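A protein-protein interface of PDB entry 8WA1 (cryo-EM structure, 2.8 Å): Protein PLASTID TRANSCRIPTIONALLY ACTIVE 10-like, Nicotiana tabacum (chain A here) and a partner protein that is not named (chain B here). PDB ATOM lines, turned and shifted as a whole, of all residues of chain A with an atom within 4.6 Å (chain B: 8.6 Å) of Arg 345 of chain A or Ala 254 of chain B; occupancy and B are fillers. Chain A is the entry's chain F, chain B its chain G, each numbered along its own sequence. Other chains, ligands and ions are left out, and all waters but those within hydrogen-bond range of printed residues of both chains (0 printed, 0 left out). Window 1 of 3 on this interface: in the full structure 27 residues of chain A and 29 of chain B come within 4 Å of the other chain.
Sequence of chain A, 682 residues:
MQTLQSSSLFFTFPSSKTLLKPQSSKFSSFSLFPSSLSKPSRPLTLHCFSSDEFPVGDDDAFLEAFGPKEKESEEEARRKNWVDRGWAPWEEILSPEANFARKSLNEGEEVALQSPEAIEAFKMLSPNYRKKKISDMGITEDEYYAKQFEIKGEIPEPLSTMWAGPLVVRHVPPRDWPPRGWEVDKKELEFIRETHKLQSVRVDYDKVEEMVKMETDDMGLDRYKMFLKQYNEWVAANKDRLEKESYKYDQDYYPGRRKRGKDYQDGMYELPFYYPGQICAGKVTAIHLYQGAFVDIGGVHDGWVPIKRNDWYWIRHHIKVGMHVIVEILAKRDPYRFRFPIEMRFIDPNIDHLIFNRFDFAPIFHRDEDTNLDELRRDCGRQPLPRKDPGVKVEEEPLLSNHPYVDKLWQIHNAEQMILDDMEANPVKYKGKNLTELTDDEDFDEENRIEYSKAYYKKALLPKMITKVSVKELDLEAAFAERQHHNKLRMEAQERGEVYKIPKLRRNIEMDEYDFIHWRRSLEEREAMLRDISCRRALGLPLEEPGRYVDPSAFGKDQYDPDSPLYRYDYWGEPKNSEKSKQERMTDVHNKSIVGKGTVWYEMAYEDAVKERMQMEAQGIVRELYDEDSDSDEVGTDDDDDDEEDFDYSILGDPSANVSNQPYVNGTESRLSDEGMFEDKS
The guanidinium group of Arg 345 of chain A lies close to the guanidinium group of Arg 251 of chain B (3.4 Å). O of Phe 255 of chain B sits at hydrogen-bond distance from NE of Arg 358 of chain A (2.9 Å). The side-chain amide nitrogen (ND2) of Asn 257 of chain B lies within hydrogen-bond range of the backbone carbonyl oxygen (O) of Asp 352 of chain A (3.2 Å). NH2 of Arg 358 of chain A lies within hydrogen-bond range of O of Ala 254 of chain B (2.8 Å).
OD1 of Asp 352 of chain A sits close to OD1 of Asn 350 of chain A. O of Glu 328 of chain A is in hydrogen-bond range of N of Arg 345 of chain A, at 2.9 Å.
NH2 of Arg 345 of chain A touches CB of Ala 254 of chain B (3.6 Å). Asp 352 of chain A touches Ala 254 of chain B.
Arg 345 of chain A touches just these residues of chain B: Arg 251 and Ala 254. Of the printed residues of chain B, Asp 352 of chain A touches Ala 254 and Asn 257. Of the printed residues of chain B, Arg 358 of chain A touches Ala 254 (2.8 Å) and Phe 255 (2.9 Å). Of the printed residues of chain A, Arg 251 of chain B touches Arg 345. Ala 254 of chain B touches just these residues of chain A: Arg 345, Asp 352 and Arg 358. Of the printed residues of chain A, Phe 255 of chain B touches Arg 358 (2.9 Å). Printed residues of chain A within 4 Å of Asn 257 of chain B: Asp 352 (3.2 Å). The nearest printed residue of chain A that does not touch Ala 254 of chain B is Asn 350 of chain A (6.0 Å).
Of the 14 printed residues of chain B, 4 touch a printed residue of chain A. Printed residues of chain B that touch a printed residue of chain A: Arg 251, Ala 254, Phe 255 and Asn 257. Along chain B the printed residues that touch a printed residue of chain A span positions 251 to 257. Among the printed residues, no Asp or Glu carboxylate lies within 4 Å of a Lys or Arg side-chain nitrogen of the other chain.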
ATOM      1  N   ILE A 326      -5.326  -8.126 -16.893  1.00  0.00           N
ATOM      2  CA  ILE A 326      -4.310  -7.274 -17.499  1.00  0.00           C
ATOM      3  C   ILE A 326      -4.096  -6.077 -16.583  1.00  0.00           C
ATOM      4  O   ILE A 326      -5.051  -5.368 -16.243  1.00  0.00           O
ATOM      5  CB  ILE A 326      -4.719  -6.821 -18.911  1.00  0.00           C
ATOM      6  CG1 ILE A 326      -4.987  -8.034 -19.803  1.00  0.00           C
ATOM      7  CG2 ILE A 326      -3.640  -5.937 -19.517  1.00  0.00           C
ATOM      8  CD1 ILE A 326      -5.446  -7.674 -21.200  1.00  0.00           C
ATOM      9  N   VAL A 327      -2.844  -5.852 -16.185  1.00  0.00           N
ATOM     10  CA  VAL A 327      -2.508  -4.829 -15.207  1.00  0.00           C
ATOM     11  C   VAL A 327      -1.477  -3.877 -15.795  1.00  0.00           C
ATOM     12  O   VAL A 327      -0.783  -4.190 -16.765  1.00  0.00           O
ATOM     13  CB  VAL A 327      -1.983  -5.445 -13.894  1.00  0.00           C
ATOM     14  CG1 VAL A 327      -3.128  -6.040 -13.096  1.00  0.00           C
ATOM     15  CG2 VAL A 327      -0.946  -6.508 -14.202  1.00  0.00           C
ATOM     16  N   GLU A 328      -1.381  -2.698 -15.183  1.00  0.00           N
ATOM     17  CA  GLU A 328      -0.443  -1.662 -15.592  1.00  0.00           C
ATOM     18  C   GLU A 328       0.341  -1.197 -14.375  1.00  0.00           C
ATOM     19  O   GLU A 328      -0.240  -0.918 -13.323  1.00  0.00           O
ATOM     20  CB  GLU A 328      -1.175  -0.477 -16.234  1.00  0.00           C
ATOM     21  CG  GLU A 328      -0.593  -0.016 -17.561  1.00  0.00           C
ATOM     22  CD  GLU A 328       0.565   0.948 -17.399  1.00  0.00           C
ATOM     23  OE1 GLU A 328       1.128   1.379 -18.427  1.00  0.00           O
ATOM     24  OE2 GLU A 328       0.908   1.283 -16.247  1.00  0.00           O
ATOM     25  N   LEU A 330       2.175   1.246 -12.095  1.00  0.00           N
ATOM     26  CA  LEU A 330       2.086   2.674 -11.812  1.00  0.00           C
ATOM     27  C   LEU A 330       3.334   3.214 -11.124  1.00  0.00           C
ATOM     28  O   LEU A 330       3.808   4.301 -11.464  1.00  0.00           O
ATOM     29  CB  LEU A 330       0.847   2.965 -10.955  1.00  0.00           C
ATOM     30  CG  LEU A 330      -0.496   2.696 -11.637  1.00  0.00           C
ATOM     31  CD1 LEU A 330      -1.651   3.045 -10.713  1.00  0.00           C
ATOM     32  CD2 LEU A 330      -0.591   3.474 -12.938  1.00  0.00           C
ATOM     33  N   MET A 344       0.049  -1.630  -9.040  1.00  0.00           N
ATOM     34  CA  MET A 344      -0.503  -1.661 -10.364  1.00  0.00           C
ATOM     35  C   MET A 344      -1.946  -1.232 -10.410  1.00  0.00           C
ATOM     36  O   MET A 344      -2.515  -0.894  -9.388  1.00  0.00           O
ATOM     37  CB  MET A 344      -0.351  -3.067 -10.901  1.00  0.00           C
ATOM     38  CG  MET A 344       1.068  -3.591 -10.874  1.00  0.00           C
ATOM     39  SD  MET A 344       1.070  -5.354 -11.163  1.00  0.00           S
ATOM     40  CE  MET A 344      -0.389  -5.809 -10.237  1.00  0.00           C
ATOM     41  N   ARG A 345      -2.539  -1.213 -11.593  1.00  0.00           N
ATOM     42  CA  ARG A 345      -3.950  -0.889 -11.726  1.00  0.00           C
ATOM     43  C   ARG A 345      -4.546  -1.923 -12.638  1.00  0.00           C
ATOM     44  O   ARG A 345      -3.847  -2.488 -13.461  1.00  0.00           O
ATOM     45  CB  ARG A 345      -4.154   0.502 -12.300  1.00  0.00           C
ATOM     46  CG  ARG A 345      -3.710   0.692 -13.737  1.00  0.00           C
ATOM     47  CD  ARG A 345      -4.171   2.043 -14.254  1.00  0.00           C
ATOM     48  NE  ARG A 345      -5.611   2.216 -14.096  1.00  0.00           N
ATOM     49  CZ  ARG A 345      -6.501   2.002 -15.059  1.00  0.00           C
ATOM     50  NH1 ARG A 345      -6.103   1.620 -16.262  1.00  0.00           N
ATOM     51  NH2 ARG A 345      -7.791   2.180 -14.820  1.00  0.00           N
ATOM     52  N   PHE A 346      -5.826  -2.208 -12.493  1.00  0.00           N
ATOM     53  CA  PHE A 346      -6.416  -3.266 -13.279  1.00  0.00           C
ATOM     54  C   PHE A 346      -6.973  -2.714 -14.550  1.00  0.00           C
ATOM     55  O   PHE A 346      -8.087  -2.215 -14.557  1.00  0.00           O
ATOM     56  CB  PHE A 346      -7.596  -3.856 -12.535  1.00  0.00           C
ATOM     57  CG  PHE A 346      -7.246  -4.919 -11.549  1.00  0.00           C
ATOM     58  CD1 PHE A 346      -6.428  -5.964 -11.896  1.00  0.00           C
ATOM     59  CD2 PHE A 346      -7.792  -4.896 -10.284  1.00  0.00           C
ATOM     60  CE1 PHE A 346      -6.125  -6.950 -10.984  1.00  0.00           C
ATOM     61  CE2 PHE A 346      -7.499  -5.879  -9.367  1.00  0.00           C
ATOM     62  CZ  PHE A 346      -6.661  -6.909  -9.718  1.00  0.00           C
ATOM     63  N   ILE A 347      -6.225  -2.785 -15.636  1.00  0.00           N
ATOM     64  CA  ILE A 347      -6.781  -2.367 -16.904  1.00  0.00           C
ATOM     65  C   ILE A 347      -7.898  -3.273 -17.383  1.00  0.00           C
ATOM     66  O   ILE A 347      -8.966  -2.800 -17.742  1.00  0.00           O
ATOM     67  CB  ILE A 347      -5.705  -2.380 -17.985  1.00  0.00           C
ATOM     68  CG1 ILE A 347      -4.650  -1.323 -17.702  1.00  0.00           C
ATOM     69  CG2 ILE A 347      -6.307  -2.148 -19.357  1.00  0.00           C
ATOM     70  CD1 ILE A 347      -3.683  -1.168 -18.848  1.00  0.00           C
ATOM     71  N   ASN A 350     -11.095  -3.172 -15.106  1.00  0.00           N
ATOM     72  CA  ASN A 350     -11.609  -1.794 -14.998  1.00  0.00           C
ATOM     73  C   ASN A 350     -12.608  -1.613 -13.882  1.00  0.00           C
ATOM     74  O   ASN A 350     -13.759  -1.308 -14.121  1.00  0.00           O
ATOM     75  CB  ASN A 350     -12.135  -1.236 -16.306  1.00  0.00           C
ATOM     76  CG  ASN A 350     -11.727   0.200 -16.509  1.00  0.00           C
ATOM     77  OD1 ASN A 350     -10.724   0.647 -15.961  1.00  0.00           O
ATOM     78  ND2 ASN A 350     -12.490   0.928 -17.300  1.00  0.00           N
ATOM     79  N   ASP A 352     -12.547   0.619 -11.594  1.00  0.00           N
ATOM     80  CA  ASP A 352     -12.400   1.940 -10.991  1.00  0.00           C
ATOM     81  C   ASP A 352     -13.644   2.655 -10.522  1.00  0.00           C
ATOM     82  O   ASP A 352     -13.571   3.485  -9.627  1.00  0.00           O
ATOM     83  CB  ASP A 352     -11.528   2.861 -11.839  1.00  0.00           C
ATOM     84  CG  ASP A 352     -11.910   2.870 -13.298  1.00  0.00           C
ATOM     85  OD1 ASP A 352     -12.339   1.827 -13.823  1.00  0.00           O
ATOM     86  OD2 ASP A 352     -11.755   3.929 -13.939  1.00  0.00           O
ATOM     87  N   ARG A 358      -8.959   5.288  -0.760  1.00  0.00           N
ATOM     88  CA  ARG A 358      -7.634   5.294  -1.357  1.00  0.00           C
ATOM     89  C   ARG A 358      -6.567   5.283  -0.271  1.00  0.00           C
ATOM     90  O   ARG A 358      -6.831   5.581   0.897  1.00  0.00           O
ATOM     91  CB  ARG A 358      -7.434   6.523  -2.257  1.00  0.00           C
ATOM     92  CG  ARG A 358      -8.497   6.707  -3.328  1.00  0.00           C
ATOM     93  CD  ARG A 358      -8.365   5.672  -4.432  1.00  0.00           C
ATOM     94  NE  ARG A 358      -9.365   5.866  -5.479  1.00  0.00           N
ATOM     95  CZ  ARG A 358      -9.436   5.139  -6.588  1.00  0.00           C
ATOM     96  NH1 ARG A 358      -8.561   4.166  -6.803  1.00  0.00           N
ATOM     97  NH2 ARG A 358     -10.381   5.385  -7.485  1.00  0.00           N
ATOM     98  N   ARG B 186      -7.382  15.497  -5.104  1.00  0.00           N
ATOM     99  CA  ARG B 186      -7.611  14.126  -4.656  1.00  0.00           C
ATOM    100  C   ARG B 186      -8.235  14.098  -3.265  1.00  0.00           C
ATOM    101  O   ARG B 186      -9.103  13.265  -2.978  1.00  0.00           O
ATOM    102  CB  ARG B 186      -6.296  13.345  -4.668  1.00  0.00           C
ATOM    103  CG  ARG B 186      -5.658  13.213  -6.040  1.00  0.00           C
ATOM    104  CD  ARG B 186      -4.383  12.389  -5.971  1.00  0.00           C
ATOM    105  NE  ARG B 186      -3.807  12.160  -7.292  1.00  0.00           N
ATOM    106  CZ  ARG B 186      -2.710  11.445  -7.518  1.00  0.00           C
ATOM    107  NH1 ARG B 186      -2.061  10.885  -6.506  1.00  0.00           N
ATOM    108  NH2 ARG B 186      -2.261  11.291  -8.755  1.00  0.00           N
ATOM    109  N   ILE B 208      -4.372  16.611 -10.217  1.00  0.00           N
ATOM    110  CA  ILE B 208      -4.453  16.211 -11.618  1.00  0.00           C
ATOM    111  C   ILE B 208      -4.839  17.444 -12.433  1.00  0.00           C
ATOM    112  O   ILE B 208      -5.984  17.910 -12.321  1.00  0.00           O
ATOM    113  CB  ILE B 208      -5.461  15.074 -11.827  1.00  0.00           C
ATOM    114  CG1 ILE B 208      -5.184  13.925 -10.856  1.00  0.00           C
ATOM    115  CG2 ILE B 208      -5.403  14.584 -13.262  1.00  0.00           C
ATOM    116  CD1 ILE B 208      -3.852  13.245 -11.076  1.00  0.00           C
ATOM    117  N   GLY B 247     -11.132  13.965 -21.402  1.00  0.00           N
ATOM    118  CA  GLY B 247     -10.333  12.748 -21.423  1.00  0.00           C
ATOM    119  C   GLY B 247      -9.404  12.643 -20.228  1.00  0.00           C
ATOM    120  O   GLY B 247      -9.254  11.572 -19.633  1.00  0.00           O
ATOM    121  N   ARG B 248      -8.760  13.755 -19.863  1.00  0.00           N
ATOM    122  CA  ARG B 248      -7.915  13.753 -18.673  1.00  0.00           C
ATOM    123  C   ARG B 248      -8.733  13.512 -17.413  1.00  0.00           C
ATOM    124  O   ARG B 248      -8.264  12.838 -16.491  1.00  0.00           O
ATOM    125  CB  ARG B 248      -7.149  15.071 -18.558  1.00  0.00           C
ATOM    126  CG  ARG B 248      -6.227  15.363 -19.726  1.00  0.00           C
ATOM    127  CD  ARG B 248      -5.609  16.741 -19.593  1.00  0.00           C
ATOM    128  NE  ARG B 248      -5.458  17.396 -20.889  1.00  0.00           N
ATOM    129  CZ  ARG B 248      -4.378  17.297 -21.656  1.00  0.00           C
ATOM    130  NH1 ARG B 248      -3.344  16.569 -21.260  1.00  0.00           N
ATOM    131  NH2 ARG B 248      -4.332  17.928 -22.822  1.00  0.00           N
ATOM    132  N   MET B 249      -9.961  14.035 -17.361  1.00  0.00           N
ATOM    133  CA  MET B 249     -10.831  13.766 -16.221  1.00  0.00           C
ATOM    134  C   MET B 249     -11.218  12.293 -16.161  1.00  0.00           C
ATOM    135  O   MET B 249     -11.244  11.694 -15.080  1.00  0.00           O
ATOM    136  CB  MET B 249     -12.077  14.647 -16.295  1.00  0.00           C
ATOM    137  CG  MET B 249     -13.116  14.347 -15.227  1.00  0.00           C
ATOM    138  SD  MET B 249     -14.536  15.453 -15.319  1.00  0.00           S
ATOM    139  CE  MET B 249     -15.601  14.752 -14.062  1.00  0.00           C
ATOM    140  N   ALA B 250     -11.520  11.693 -17.314  1.00  0.00           N
ATOM    141  CA  ALA B 250     -11.840  10.269 -17.343  1.00  0.00           C
ATOM    142  C   ALA B 250     -10.644   9.430 -16.912  1.00  0.00           C
ATOM    143  O   ALA B 250     -10.802   8.418 -16.220  1.00  0.00           O
ATOM    144  CB  ALA B 250     -12.307   9.864 -18.741  1.00  0.00           C
ATOM    145  N   ARG B 251      -9.439   9.836 -17.314  1.00  0.00           N
ATOM    146  CA  ARG B 251      -8.235   9.135 -16.880  1.00  0.00           C
ATOM    147  C   ARG B 251      -8.016   9.288 -15.380  1.00  0.00           C
ATOM    148  O   ARG B 251      -7.615   8.335 -14.701  1.00  0.00           O
ATOM    149  CB  ARG B 251      -7.024   9.651 -17.657  1.00  0.00           C
ATOM    150  CG  ARG B 251      -5.707   9.018 -17.249  1.00  0.00           C
ATOM    151  CD  ARG B 251      -5.738   7.512 -17.439  1.00  0.00           C
ATOM    152  NE  ARG B 251      -4.502   6.883 -16.984  1.00  0.00           N
ATOM    153  CZ  ARG B 251      -4.292   5.572 -16.973  1.00  0.00           C
ATOM    154  NH1 ARG B 251      -3.136   5.088 -16.541  1.00  0.00           N
ATOM    155  NH2 ARG B 251      -5.238   4.743 -17.392  1.00  0.00           N
ATOM    156  N   ALA B 252      -8.272  10.484 -14.844  1.00  0.00           N
ATOM    157  CA  ALA B 252      -8.086  10.718 -13.416  1.00  0.00           C
ATOM    158  C   ALA B 252      -9.148  10.015 -12.584  1.00  0.00           C
ATOM    159  O   ALA B 252      -8.924   9.741 -11.398  1.00  0.00           O
ATOM    160  CB  ALA B 252      -8.096  12.218 -13.124  1.00  0.00           C
ATOM    161  N   GLN B 253     -10.309   9.726 -13.178  1.00  0.00           N
ATOM    162  CA  GLN B 253     -11.370   9.040 -12.447  1.00  0.00           C
ATOM    163  C   GLN B 253     -10.917   7.696 -11.895  1.00  0.00           C
ATOM    164  O   GLN B 253     -11.500   7.213 -10.919  1.00  0.00           O
ATOM    165  CB  GLN B 253     -12.594   8.847 -13.343  1.00  0.00           C
ATOM    166  CG  GLN B 253     -13.483  10.073 -13.463  1.00  0.00           C
ATOM    167  CD  GLN B 253     -14.718   9.812 -14.300  1.00  0.00           C
ATOM    168  OE1 GLN B 253     -15.643  10.624 -14.334  1.00  0.00           O
ATOM    169  NE2 GLN B 253     -14.739   8.674 -14.983  1.00  0.00           N
ATOM    170  N   ALA B 254      -9.892   7.085 -12.491  1.00  0.00           N
ATOM    171  CA  ALA B 254      -9.325   5.870 -11.916  1.00  0.00           C
ATOM    172  C   ALA B 254      -8.624   6.168 -10.597  1.00  0.00           C
ATOM    173  O   ALA B 254      -8.681   5.372  -9.654  1.00  0.00           O
ATOM    174  CB  ALA B 254      -8.364   5.218 -12.911  1.00  0.00           C
ATOM    175  N   PHE B 255      -7.958   7.324 -10.514  1.00  0.00           N
ATOM    176  CA  PHE B 255      -7.239   7.679  -9.294  1.00  0.00           C
ATOM    177  C   PHE B 255      -8.173   8.287  -8.255  1.00  0.00           C
ATOM    178  O   PHE B 255      -8.127   7.912  -7.078  1.00  0.00           O
ATOM    179  CB  PHE B 255      -6.100   8.643  -9.623  1.00  0.00           C
ATOM    180  CG  PHE B 255      -5.199   8.161 -10.722  1.00  0.00           C
ATOM    181  CD1 PHE B 255      -4.178   7.265 -10.456  1.00  0.00           C
ATOM    182  CD2 PHE B 255      -5.374   8.604 -12.023  1.00  0.00           C
ATOM    183  CE1 PHE B 255      -3.349   6.817 -11.467  1.00  0.00           C
ATOM    184  CE2 PHE B 255      -4.548   8.161 -13.037  1.00  0.00           C
ATOM    185  CZ  PHE B 255      -3.535   7.267 -12.758  1.00  0.00           C
ATOM    186  N   VAL B 256      -9.021   9.227  -8.665  1.00  0.00           N
ATOM    187  CA  VAL B 256      -9.975   9.878  -7.775  1.00  0.00           C
ATOM    188  C   VAL B 256     -11.379   9.623  -8.306  1.00  0.00           C
ATOM    189  O   VAL B 256     -11.689   9.977  -9.448  1.00  0.00           O
ATOM    190  CB  VAL B 256      -9.702  11.391  -7.646  1.00  0.00           C
ATOM    191  CG1 VAL B 256      -9.363  11.997  -9.002  1.00  0.00           C
ATOM    192  CG2 VAL B 256     -10.899  12.096  -7.026  1.00  0.00           C
ATOM    193  N   ASN B 257     -12.222   9.008  -7.479  1.00  0.00           N
ATOM    194  CA  ASN B 257     -13.573   8.623  -7.875  1.00  0.00           C
ATOM    195  C   ASN B 257     -14.521   9.763  -7.523  1.00  0.00           C
ATOM    196  O   ASN B 257     -14.666  10.120  -6.349  1.00  0.00           O
ATOM    197  CB  ASN B 257     -13.990   7.324  -7.190  1.00  0.00           C
ATOM    198  CG  ASN B 257     -15.235   6.707  -7.804  1.00  0.00           C
ATOM    199  OD1 ASN B 257     -16.092   7.405  -8.345  1.00  0.00           O
ATOM    200  ND2 ASN B 257     -15.339   5.385  -7.722  1.00  0.00           N
ATOM    201  N   LEU B 258     -15.164  10.331  -8.541  1.00  0.00           N
ATOM    202  CA  LEU B 258     -16.123  11.420  -8.364  1.00  0.00           C
ATOM    203  C   LEU B 258     -17.525  10.826  -8.460  1.00  0.00           C
ATOM    204  O   LEU B 258     -18.144  10.811  -9.523  1.00  0.00           O
ATOM    205  CB  LEU B 258     -15.899  12.514  -9.402  1.00  0.00           C
ATOM    206  CG  LEU B 258     -14.542  13.217  -9.368  1.00  0.00           C
ATOM    207  CD1 LEU B 258     -14.439  14.234 -10.492  1.00  0.00           C
ATOM    208  CD2 LEU B 258     -14.320  13.881  -8.018  1.00  0.00           C
